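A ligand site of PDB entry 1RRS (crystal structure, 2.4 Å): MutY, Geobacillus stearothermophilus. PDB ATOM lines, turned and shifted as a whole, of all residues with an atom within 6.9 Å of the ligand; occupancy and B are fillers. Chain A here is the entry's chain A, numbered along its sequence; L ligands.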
ATOM      1  N   ARG A 152      13.136   8.668   1.322  1.00  0.00           N
ATOM      2  CA  ARG A 152      11.801   8.464   1.895  1.00  0.00           C
ATOM      3  C   ARG A 152      11.353   7.021   1.630  1.00  0.00           C
ATOM      4  O   ARG A 152      10.799   6.360   2.505  1.00  0.00           O
ATOM      5  CB  ARG A 152      10.794   9.429   1.276  1.00  0.00           C
ATOM      6  CG  ARG A 152       9.384   9.223   1.826  1.00  0.00           C
ATOM      7  CD  ARG A 152       8.432  10.334   1.404  1.00  0.00           C
ATOM      8  NE  ARG A 152       8.253  10.364  -0.051  1.00  0.00           N
ATOM      9  CZ  ARG A 152       8.870  11.210  -0.870  1.00  0.00           C
ATOM     10  NH1 ARG A 152       9.710  12.119  -0.385  1.00  0.00           N
ATOM     11  NH2 ARG A 152       8.659  11.141  -2.169  1.00  0.00           N
ATOM     12  N   VAL A 153      11.603   6.547   0.421  1.00  0.00           N
ATOM     13  CA  VAL A 153      11.216   5.200   0.062  1.00  0.00           C
ATOM     14  C   VAL A 153      12.006   4.151   0.835  1.00  0.00           C
ATOM     15  O   VAL A 153      11.438   3.215   1.388  1.00  0.00           O
ATOM     16  CB  VAL A 153      11.416   4.964  -1.451  1.00  0.00           C
ATOM     17  CG1 VAL A 153      11.311   3.484  -1.774  1.00  0.00           C
ATOM     18  CG2 VAL A 153      10.387   5.759  -2.220  1.00  0.00           C
ATOM     19  N   LEU A 154      13.319   4.303   0.858  1.00  0.00           N
ATOM     20  CA  LEU A 154      14.188   3.366   1.557  1.00  0.00           C
ATOM     21  C   LEU A 154      13.995   3.394   3.066  1.00  0.00           C
ATOM     22  O   LEU A 154      14.112   2.356   3.720  1.00  0.00           O
ATOM     23  CB  LEU A 154      15.646   3.673   1.212  1.00  0.00           C
ATOM     24  CG  LEU A 154      16.077   3.381  -0.218  1.00  0.00           C
ATOM     25  CD1 LEU A 154      17.573   3.651  -0.354  1.00  0.00           C
ATOM     26  CD2 LEU A 154      15.788   1.938  -0.564  1.00  0.00           C
ATOM     27  N   ARG A 156      11.323   3.793   4.524  1.00  0.00           N
ATOM     28  CA  ARG A 156      10.081   3.075   4.791  1.00  0.00           C
ATOM     29  C   ARG A 156      10.235   1.590   4.535  1.00  0.00           C
ATOM     30  O   ARG A 156       9.887   0.765   5.387  1.00  0.00           O
ATOM     31  CB  ARG A 156       8.939   3.649   3.926  1.00  0.00           C
ATOM     32  CG  ARG A 156       8.381   4.942   4.467  1.00  0.00           C
ATOM     33  CD  ARG A 156       7.638   5.692   3.388  1.00  0.00           C
ATOM     34  NE  ARG A 156       7.019   6.914   3.911  1.00  0.00           N
ATOM     35  CZ  ARG A 156       6.275   7.735   3.187  1.00  0.00           C
ATOM     36  NH1 ARG A 156       6.045   7.470   1.908  1.00  0.00           N
ATOM     37  NH2 ARG A 156       5.722   8.808   3.759  1.00  0.00           N
ATOM     38  N   LEU A 157      10.754   1.233   3.361  1.00  0.00           N
ATOM     39  CA  LEU A 157      10.943  -0.165   3.041  1.00  0.00           C
ATOM     40  C   LEU A 157      11.719  -0.853   4.140  1.00  0.00           C
ATOM     41  O   LEU A 157      11.281  -1.873   4.669  1.00  0.00           O
ATOM     42  CB  LEU A 157      11.696  -0.306   1.713  1.00  0.00           C
ATOM     43  CG  LEU A 157      10.872   0.068   0.491  1.00  0.00           C
ATOM     44  CD1 LEU A 157      11.762   0.029  -0.744  1.00  0.00           C
ATOM     45  CD2 LEU A 157       9.696  -0.887   0.353  1.00  0.00           C
ATOM     46  N   LEU A 196       8.751   5.964  -7.956  1.00  0.00           N
ATOM     47  CA  LEU A 196       7.942   5.394  -6.878  1.00  0.00           C
ATOM     48  C   LEU A 196       7.739   6.443  -5.805  1.00  0.00           C
ATOM     49  O   LEU A 196       6.619   6.702  -5.380  1.00  0.00           O
ATOM     50  CB  LEU A 196       8.612   4.155  -6.263  1.00  0.00           C
ATOM     51  CG  LEU A 196       7.658   3.326  -5.386  1.00  0.00           C
ATOM     52  CD1 LEU A 196       6.653   2.601  -6.290  1.00  0.00           C
ATOM     53  CD2 LEU A 196       8.426   2.309  -4.554  1.00  0.00           C
ATOM     54  N   VAL A 200       3.957   7.057  -5.964  1.00  0.00           N
ATOM     55  CA  VAL A 200       3.332   6.201  -4.953  1.00  0.00           C
ATOM     56  C   VAL A 200       3.667   6.566  -3.502  1.00  0.00           C
ATOM     57  O   VAL A 200       2.833   7.082  -2.758  1.00  0.00           O
ATOM     58  CB  VAL A 200       3.713   4.704  -5.196  1.00  0.00           C
ATOM     59  CG1 VAL A 200       2.925   3.809  -4.252  1.00  0.00           C
ATOM     60  CG2 VAL A 200       3.446   4.317  -6.638  1.00  0.00           C
ATOM     61  N   CYS A 201       4.914   6.274  -3.107  1.00  0.00           N
ATOM     62  CA  CYS A 201       5.402   6.535  -1.759  1.00  0.00           C
ATOM     63  C   CYS A 201       5.645   8.009  -1.522  1.00  0.00           C
ATOM     64  O   CYS A 201       6.767   8.450  -1.291  1.00  0.00           O
ATOM     65  CB  CYS A 201       6.691   5.728  -1.539  1.00  0.00           C
ATOM     66  SG  CYS A 201       7.207   5.626   0.190  1.00  0.00           S
ATOM     67  N   THR A 202       4.569   8.783  -1.573  1.00  0.00           N
ATOM     68  CA  THR A 202       4.597  10.223  -1.394  1.00  0.00           C
ATOM     69  C   THR A 202       4.842  10.634   0.050  1.00  0.00           C
ATOM     70  O   THR A 202       4.661   9.838   0.984  1.00  0.00           O
ATOM     71  CB  THR A 202       3.259  10.813  -1.842  1.00  0.00           C
ATOM     72  OG1 THR A 202       2.195  10.065  -1.246  1.00  0.00           O
ATOM     73  CG2 THR A 202       3.140  10.760  -3.366  1.00  0.00           C
ATOM     74  N   PRO A 206       0.908   8.064   1.730  1.00  0.00           N
ATOM     75  CA  PRO A 206       1.475   7.148   0.735  1.00  0.00           C
ATOM     76  C   PRO A 206       0.422   6.127   0.304  1.00  0.00           C
ATOM     77  O   PRO A 206      -0.321   5.608   1.144  1.00  0.00           O
ATOM     78  CB  PRO A 206       2.651   6.516   1.476  1.00  0.00           C
ATOM     79  CG  PRO A 206       2.183   6.523   2.896  1.00  0.00           C
ATOM     80  CD  PRO A 206       1.571   7.888   3.037  1.00  0.00           C
ATOM     81  N   SER A 207       0.348   5.860  -0.993  1.00  0.00           N
ATOM     82  CA  SER A 207      -0.641   4.904  -1.498  1.00  0.00           C
ATOM     83  C   SER A 207      -0.097   3.489  -1.444  1.00  0.00           C
ATOM     84  O   SER A 207       0.109   2.838  -2.462  1.00  0.00           O
ATOM     85  CB  SER A 207      -1.016   5.271  -2.934  1.00  0.00           C
ATOM     86  OG  SER A 207      -1.492   6.613  -2.992  1.00  0.00           O
ATOM     87  N   CYS A 208       0.130   3.032  -0.213  1.00  0.00           N
ATOM     88  CA  CYS A 208       0.667   1.701   0.048  1.00  0.00           C
ATOM     89  C   CYS A 208      -0.183   0.573  -0.540  1.00  0.00           C
ATOM     90  O   CYS A 208       0.342  -0.440  -1.010  1.00  0.00           O
ATOM     91  CB  CYS A 208       0.828   1.526   1.565  1.00  0.00           C
ATOM     92  SG  CYS A 208       1.609   2.960   2.375  1.00  0.00           S
ATOM     93  N   LEU A 209      -1.500   0.742  -0.522  1.00  0.00           N
ATOM     94  CA  LEU A 209      -2.377  -0.270  -1.070  1.00  0.00           C
ATOM     95  C   LEU A 209      -2.096  -0.544  -2.553  1.00  0.00           C
ATOM     96  O   LEU A 209      -2.168  -1.684  -3.001  1.00  0.00           O
ATOM     97  CB  LEU A 209      -3.843   0.140  -0.889  1.00  0.00           C
ATOM     98  CG  LEU A 209      -4.276   0.283   0.574  1.00  0.00           C
ATOM     99  CD1 LEU A 209      -5.770   0.552   0.648  1.00  0.00           C
ATOM    100  CD2 LEU A 209      -3.922  -0.988   1.329  1.00  0.00           C
ATOM    101  N   LEU A 210      -1.768   0.501  -3.301  1.00  0.00           N
ATOM    102  CA  LEU A 210      -1.472   0.355  -4.719  1.00  0.00           C
ATOM    103  C   LEU A 210       0.016   0.135  -5.012  1.00  0.00           C
ATOM    104  O   LEU A 210       0.380  -0.264  -6.127  1.00  0.00           O
ATOM    105  CB  LEU A 210      -1.963   1.584  -5.494  1.00  0.00           C
ATOM    106  N   CYS A 211       0.877   0.370  -4.029  1.00  0.00           N
ATOM    107  CA  CYS A 211       2.313   0.213  -4.225  1.00  0.00           C
ATOM    108  C   CYS A 211       2.752  -1.196  -4.647  1.00  0.00           C
ATOM    109  O   CYS A 211       2.306  -2.188  -4.090  1.00  0.00           O
ATOM    110  CB  CYS A 211       3.077   0.617  -2.964  1.00  0.00           C
ATOM    111  SG  CYS A 211       4.844   0.257  -3.065  1.00  0.00           S
ATOM    112  N   PRO A 212       3.657  -1.281  -5.629  1.00  0.00           N
ATOM    113  CA  PRO A 212       4.194  -2.550  -6.154  1.00  0.00           C
ATOM    114  C   PRO A 212       5.260  -3.211  -5.286  1.00  0.00           C
ATOM    115  O   PRO A 212       5.830  -4.233  -5.682  1.00  0.00           O
ATOM    116  CB  PRO A 212       4.725  -2.141  -7.515  1.00  0.00           C
ATOM    117  CG  PRO A 212       5.274  -0.781  -7.243  1.00  0.00           C
ATOM    118  CD  PRO A 212       4.168  -0.144  -6.423  1.00  0.00           C
ATOM    119  N   VAL A 213       5.558  -2.646  -4.126  1.00  0.00           N
ATOM    120  CA  VAL A 213       6.562  -3.254  -3.267  1.00  0.00           C
ATOM    121  C   VAL A 213       6.129  -3.278  -1.815  1.00  0.00           C
ATOM    122  O   VAL A 213       6.959  -3.333  -0.906  1.00  0.00           O
ATOM    123  CB  VAL A 213       7.919  -2.524  -3.407  1.00  0.00           C
ATOM    124  CG1 VAL A 213       8.520  -2.849  -4.771  1.00  0.00           C
ATOM    125  CG2 VAL A 213       7.742  -1.033  -3.249  1.00  0.00           C
ATOM    126  N   GLN A 214       4.823  -3.248  -1.615  1.00  0.00           N
ATOM    127  CA  GLN A 214       4.234  -3.297  -0.288  1.00  0.00           C
ATOM    128  C   GLN A 214       4.697  -4.572   0.397  1.00  0.00           C
ATOM    129  O   GLN A 214       5.019  -4.589   1.587  1.00  0.00           O
ATOM    130  CB  GLN A 214       2.705  -3.304  -0.407  1.00  0.00           C
ATOM    131  CG  GLN A 214       1.998  -3.868   0.799  1.00  0.00           C
ATOM    132  CD  GLN A 214       0.535  -4.132   0.536  1.00  0.00           C
ATOM    133  OE1 GLN A 214      -0.276  -3.198   0.407  1.00  0.00           O
ATOM    134  NE2 GLN A 214       0.178  -5.407   0.438  1.00  0.00           N
ATOM    135  N   ALA A 215       4.712  -5.651  -0.374  1.00  0.00           N
ATOM    136  CA  ALA A 215       5.132  -6.943   0.121  1.00  0.00           C
ATOM    137  C   ALA A 215       6.424  -6.858   0.924  1.00  0.00           C
ATOM    138  O   ALA A 215       6.578  -7.520   1.951  1.00  0.00           O
ATOM    139  CB  ALA A 215       5.299  -7.917  -1.040  1.00  0.00           C
ATOM    140  N   TYR A 216       7.362  -6.040   0.459  1.00  0.00           N
ATOM    141  CA  TYR A 216       8.660  -5.906   1.120  1.00  0.00           C
ATOM    142  C   TYR A 216       8.762  -4.757   2.119  1.00  0.00           C
ATOM    143  O   TYR A 216       9.780  -4.628   2.798  1.00  0.00           O
ATOM    144  CB  TYR A 216       9.774  -5.723   0.086  1.00  0.00           C
ATOM    145  CG  TYR A 216       9.644  -6.556  -1.174  1.00  0.00           C
ATOM    146  CD1 TYR A 216       8.612  -6.312  -2.087  1.00  0.00           C
ATOM    147  CD2 TYR A 216      10.566  -7.565  -1.458  1.00  0.00           C
ATOM    148  CE1 TYR A 216       8.521  -7.063  -3.264  1.00  0.00           C
ATOM    149  CE2 TYR A 216      10.469  -8.317  -2.627  1.00  0.00           C
ATOM    150  CZ  TYR A 216       9.448  -8.061  -3.526  1.00  0.00           C
ATOM    151  OH  TYR A 216       9.348  -8.804  -4.681  1.00  0.00           O
ATOM    152  N   CYS A 217       7.719  -3.937   2.230  1.00  0.00           N
ATOM    153  CA  CYS A 217       7.788  -2.795   3.131  1.00  0.00           C
ATOM    154  C   CYS A 217       7.472  -2.993   4.615  1.00  0.00           C
ATOM    155  O   CYS A 217       6.333  -3.243   5.005  1.00  0.00           O
ATOM    156  CB  CYS A 217       6.923  -1.652   2.605  1.00  0.00           C
ATOM    157  SG  CYS A 217       7.087  -0.180   3.619  1.00  0.00           S
ATOM    158  N   GLN A 218       8.511  -2.832   5.443  1.00  0.00           N
ATOM    159  CA  GLN A 218       8.385  -2.980   6.887  1.00  0.00           C
ATOM    160  C   GLN A 218       7.536  -1.899   7.536  1.00  0.00           C
ATOM    161  O   GLN A 218       6.798  -2.158   8.487  1.00  0.00           O
ATOM    162  CB  GLN A 218       9.770  -2.985   7.526  1.00  0.00           C
ATOM    163  CG  GLN A 218      10.637  -4.132   7.074  1.00  0.00           C
ATOM    164  CD  GLN A 218      12.047  -4.042   7.628  1.00  0.00           C
ATOM    165  OE1 GLN A 218      12.233  -3.840   8.838  1.00  0.00           O
ATOM    166  NE2 GLN A 218      13.034  -4.179   6.753  1.00  0.00           N
ATOM    167  N   ALA A 219       7.635  -0.673   7.041  1.00  0.00           N
ATOM    168  CA  ALA A 219       6.868   0.438   7.592  1.00  0.00           C
ATOM    169  C   ALA A 219       5.376   0.162   7.409  1.00  0.00           C
ATOM    170  O   ALA A 219       4.561   0.501   8.262  1.00  0.00           O
ATOM    171  CB  ALA A 219       7.248   1.750   6.903  1.00  0.00           C
ATOM    172  N   PHE A 220       5.035  -0.449   6.279  1.00  0.00           N
ATOM    173  CA  PHE A 220       3.643  -0.796   6.010  1.00  0.00           C
ATOM    174  C   PHE A 220       3.193  -1.858   6.999  1.00  0.00           C
ATOM    175  O   PHE A 220       2.154  -1.718   7.644  1.00  0.00           O
ATOM    176  CB  PHE A 220       3.489  -1.326   4.594  1.00  0.00           C
ATOM    177  CG  PHE A 220       2.103  -1.795   4.280  1.00  0.00           C
ATOM    178  CD1 PHE A 220       1.035  -0.895   4.273  1.00  0.00           C
ATOM    179  CD2 PHE A 220       1.846  -3.136   4.018  1.00  0.00           C
ATOM    180  CE1 PHE A 220      -0.262  -1.327   4.018  1.00  0.00           C
ATOM    181  CE2 PHE A 220       0.551  -3.578   3.748  1.00  0.00           C
ATOM    182  CZ  PHE A 220      -0.510  -2.676   3.748  1.00  0.00           C
ATOM    183  N   VAL A 224       3.543   2.415  10.148  1.00  0.00           N
ATOM    184  CA  VAL A 224       4.194   3.692  10.440  1.00  0.00           C
ATOM    185  C   VAL A 224       4.666   4.476   9.210  1.00  0.00           C
ATOM    186  O   VAL A 224       5.374   5.472   9.344  1.00  0.00           O
ATOM    187  CB  VAL A 224       5.395   3.459  11.377  1.00  0.00           C
ATOM    188  CG1 VAL A 224       4.898   2.863  12.682  1.00  0.00           C
ATOM    189  CG2 VAL A 224       6.395   2.531  10.714  1.00  0.00           C
ATOM    190  N   ALA A 225       4.256   4.024   8.032  1.00  0.00           N
ATOM    191  CA  ALA A 225       4.641   4.655   6.777  1.00  0.00           C
ATOM    192  C   ALA A 225       4.588   6.192   6.772  1.00  0.00           C
ATOM    193  O   ALA A 225       5.518   6.851   6.318  1.00  0.00           O
ATOM    194  CB  ALA A 225       3.789   4.104   5.640  1.00  0.00           C
ATOM    195  N   GLU A 226       3.490   6.749   7.279  1.00  0.00           N
ATOM    196  CA  GLU A 226       3.296   8.198   7.303  1.00  0.00           C
ATOM    197  C   GLU A 226       4.207   8.932   8.290  1.00  0.00           C
ATOM    198  O   GLU A 226       4.357  10.147   8.210  1.00  0.00           O
ATOM    199  CB  GLU A 226       1.838   8.542   7.631  1.00  0.00           C
ATOM    200  CG  GLU A 226       0.850   7.446   7.259  1.00  0.00           C
ATOM    201  CD  GLU A 226       1.029   6.179   8.096  1.00  0.00           C
ATOM    202  OE1 GLU A 226       0.802   6.239   9.331  1.00  0.00           O
ATOM    203  OE2 GLU A 226       1.400   5.122   7.536  1.00  0.00           O
HETATM  204 FE1  LIG L   1       5.054   1.307  -0.800  1.00  0.00          FE
HETATM  205 FE2  LIG L   1       6.088   3.421   0.537  1.00  0.00          FE
HETATM  206 FE3  LIG L   1       3.714   2.228   1.345  1.00  0.00          FE
HETATM  207 FE4  LIG L   1       6.092   1.089   1.722  1.00  0.00          FE
HETATM  208  S1  LIG L   1       5.367   3.027   2.668  1.00  0.00           S
HETATM  209  S2  LIG L   1       4.216   0.333   1.003  1.00  0.00           S
HETATM  210  S3  LIG L   1       7.211   1.777  -0.146  1.00  0.00           S
HETATM  211  S4  LIG L   1       4.083   3.270  -0.588  1.00  0.00           S
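SG of Cys 208 is bound to FE3 of the ligand, at 2.5 Å. The side-chain sulfur (SG) of Cys 217 binds an iron atom (FE4) of the ligand (2.5 Å). SG of Cys 201 is bound to FE2 of the ligand, 2.5 Å away. SG of Cys 211 is bound to FE1 of the ligand (2.5 Å).
O of Cys 208 lies close to OE1 of Gln 214 (3.2 Å). The side-chain sulfur (SG) of Cys 208 sits close to the backbone carbonyl oxygen (O) of Pro 206 (3.5 Å). SG of Cys 217 sits close to N of Ala 219 (3.5 Å). O of Cys 201 is in hydrogen-bond range of NH1 of Arg 156. N of Gln 214 lies close to SG of Cys 211, 3.8 Å away. The side-chain sulfur of Cys 211 lies close to the backbone NH of Val 213, at 3.2 Å. The backbone carbonyl oxygen (O) of Thr 202 lies within hydrogen-bond range of the guanidinium group (NH1) of Arg 156 (2.9 Å). The backbone carbonyl oxygen (O) of Leu 157 lies within hydrogen-bond range of the backbone NH (N) of Gln 218 (3.0 Å).
Arg 156 touches the ligand (CD to S1, 3.6 Å). CD2 of Leu 157 touches S3 of the ligand, 3.7 Å away. Val 200 touches the ligand. CA of Gln 214 touches S2 of the ligand (3.9 Å). Ala 225 touches the ligand (CB to S1, 3.5 Å). Hydrophobic or aromatic side chains within 4 Å of the ligand: Leu 157, Val 200 and Ala 225. Within 4 Å of the ligand: Arg 156, Leu 157, Val 200, Cys 201, Cys 208, Cys 211, Gln 214, Cys 217 and Ala 225. The nearest printed residue that does not touch the ligand is Phe 220 (4.02 Å).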
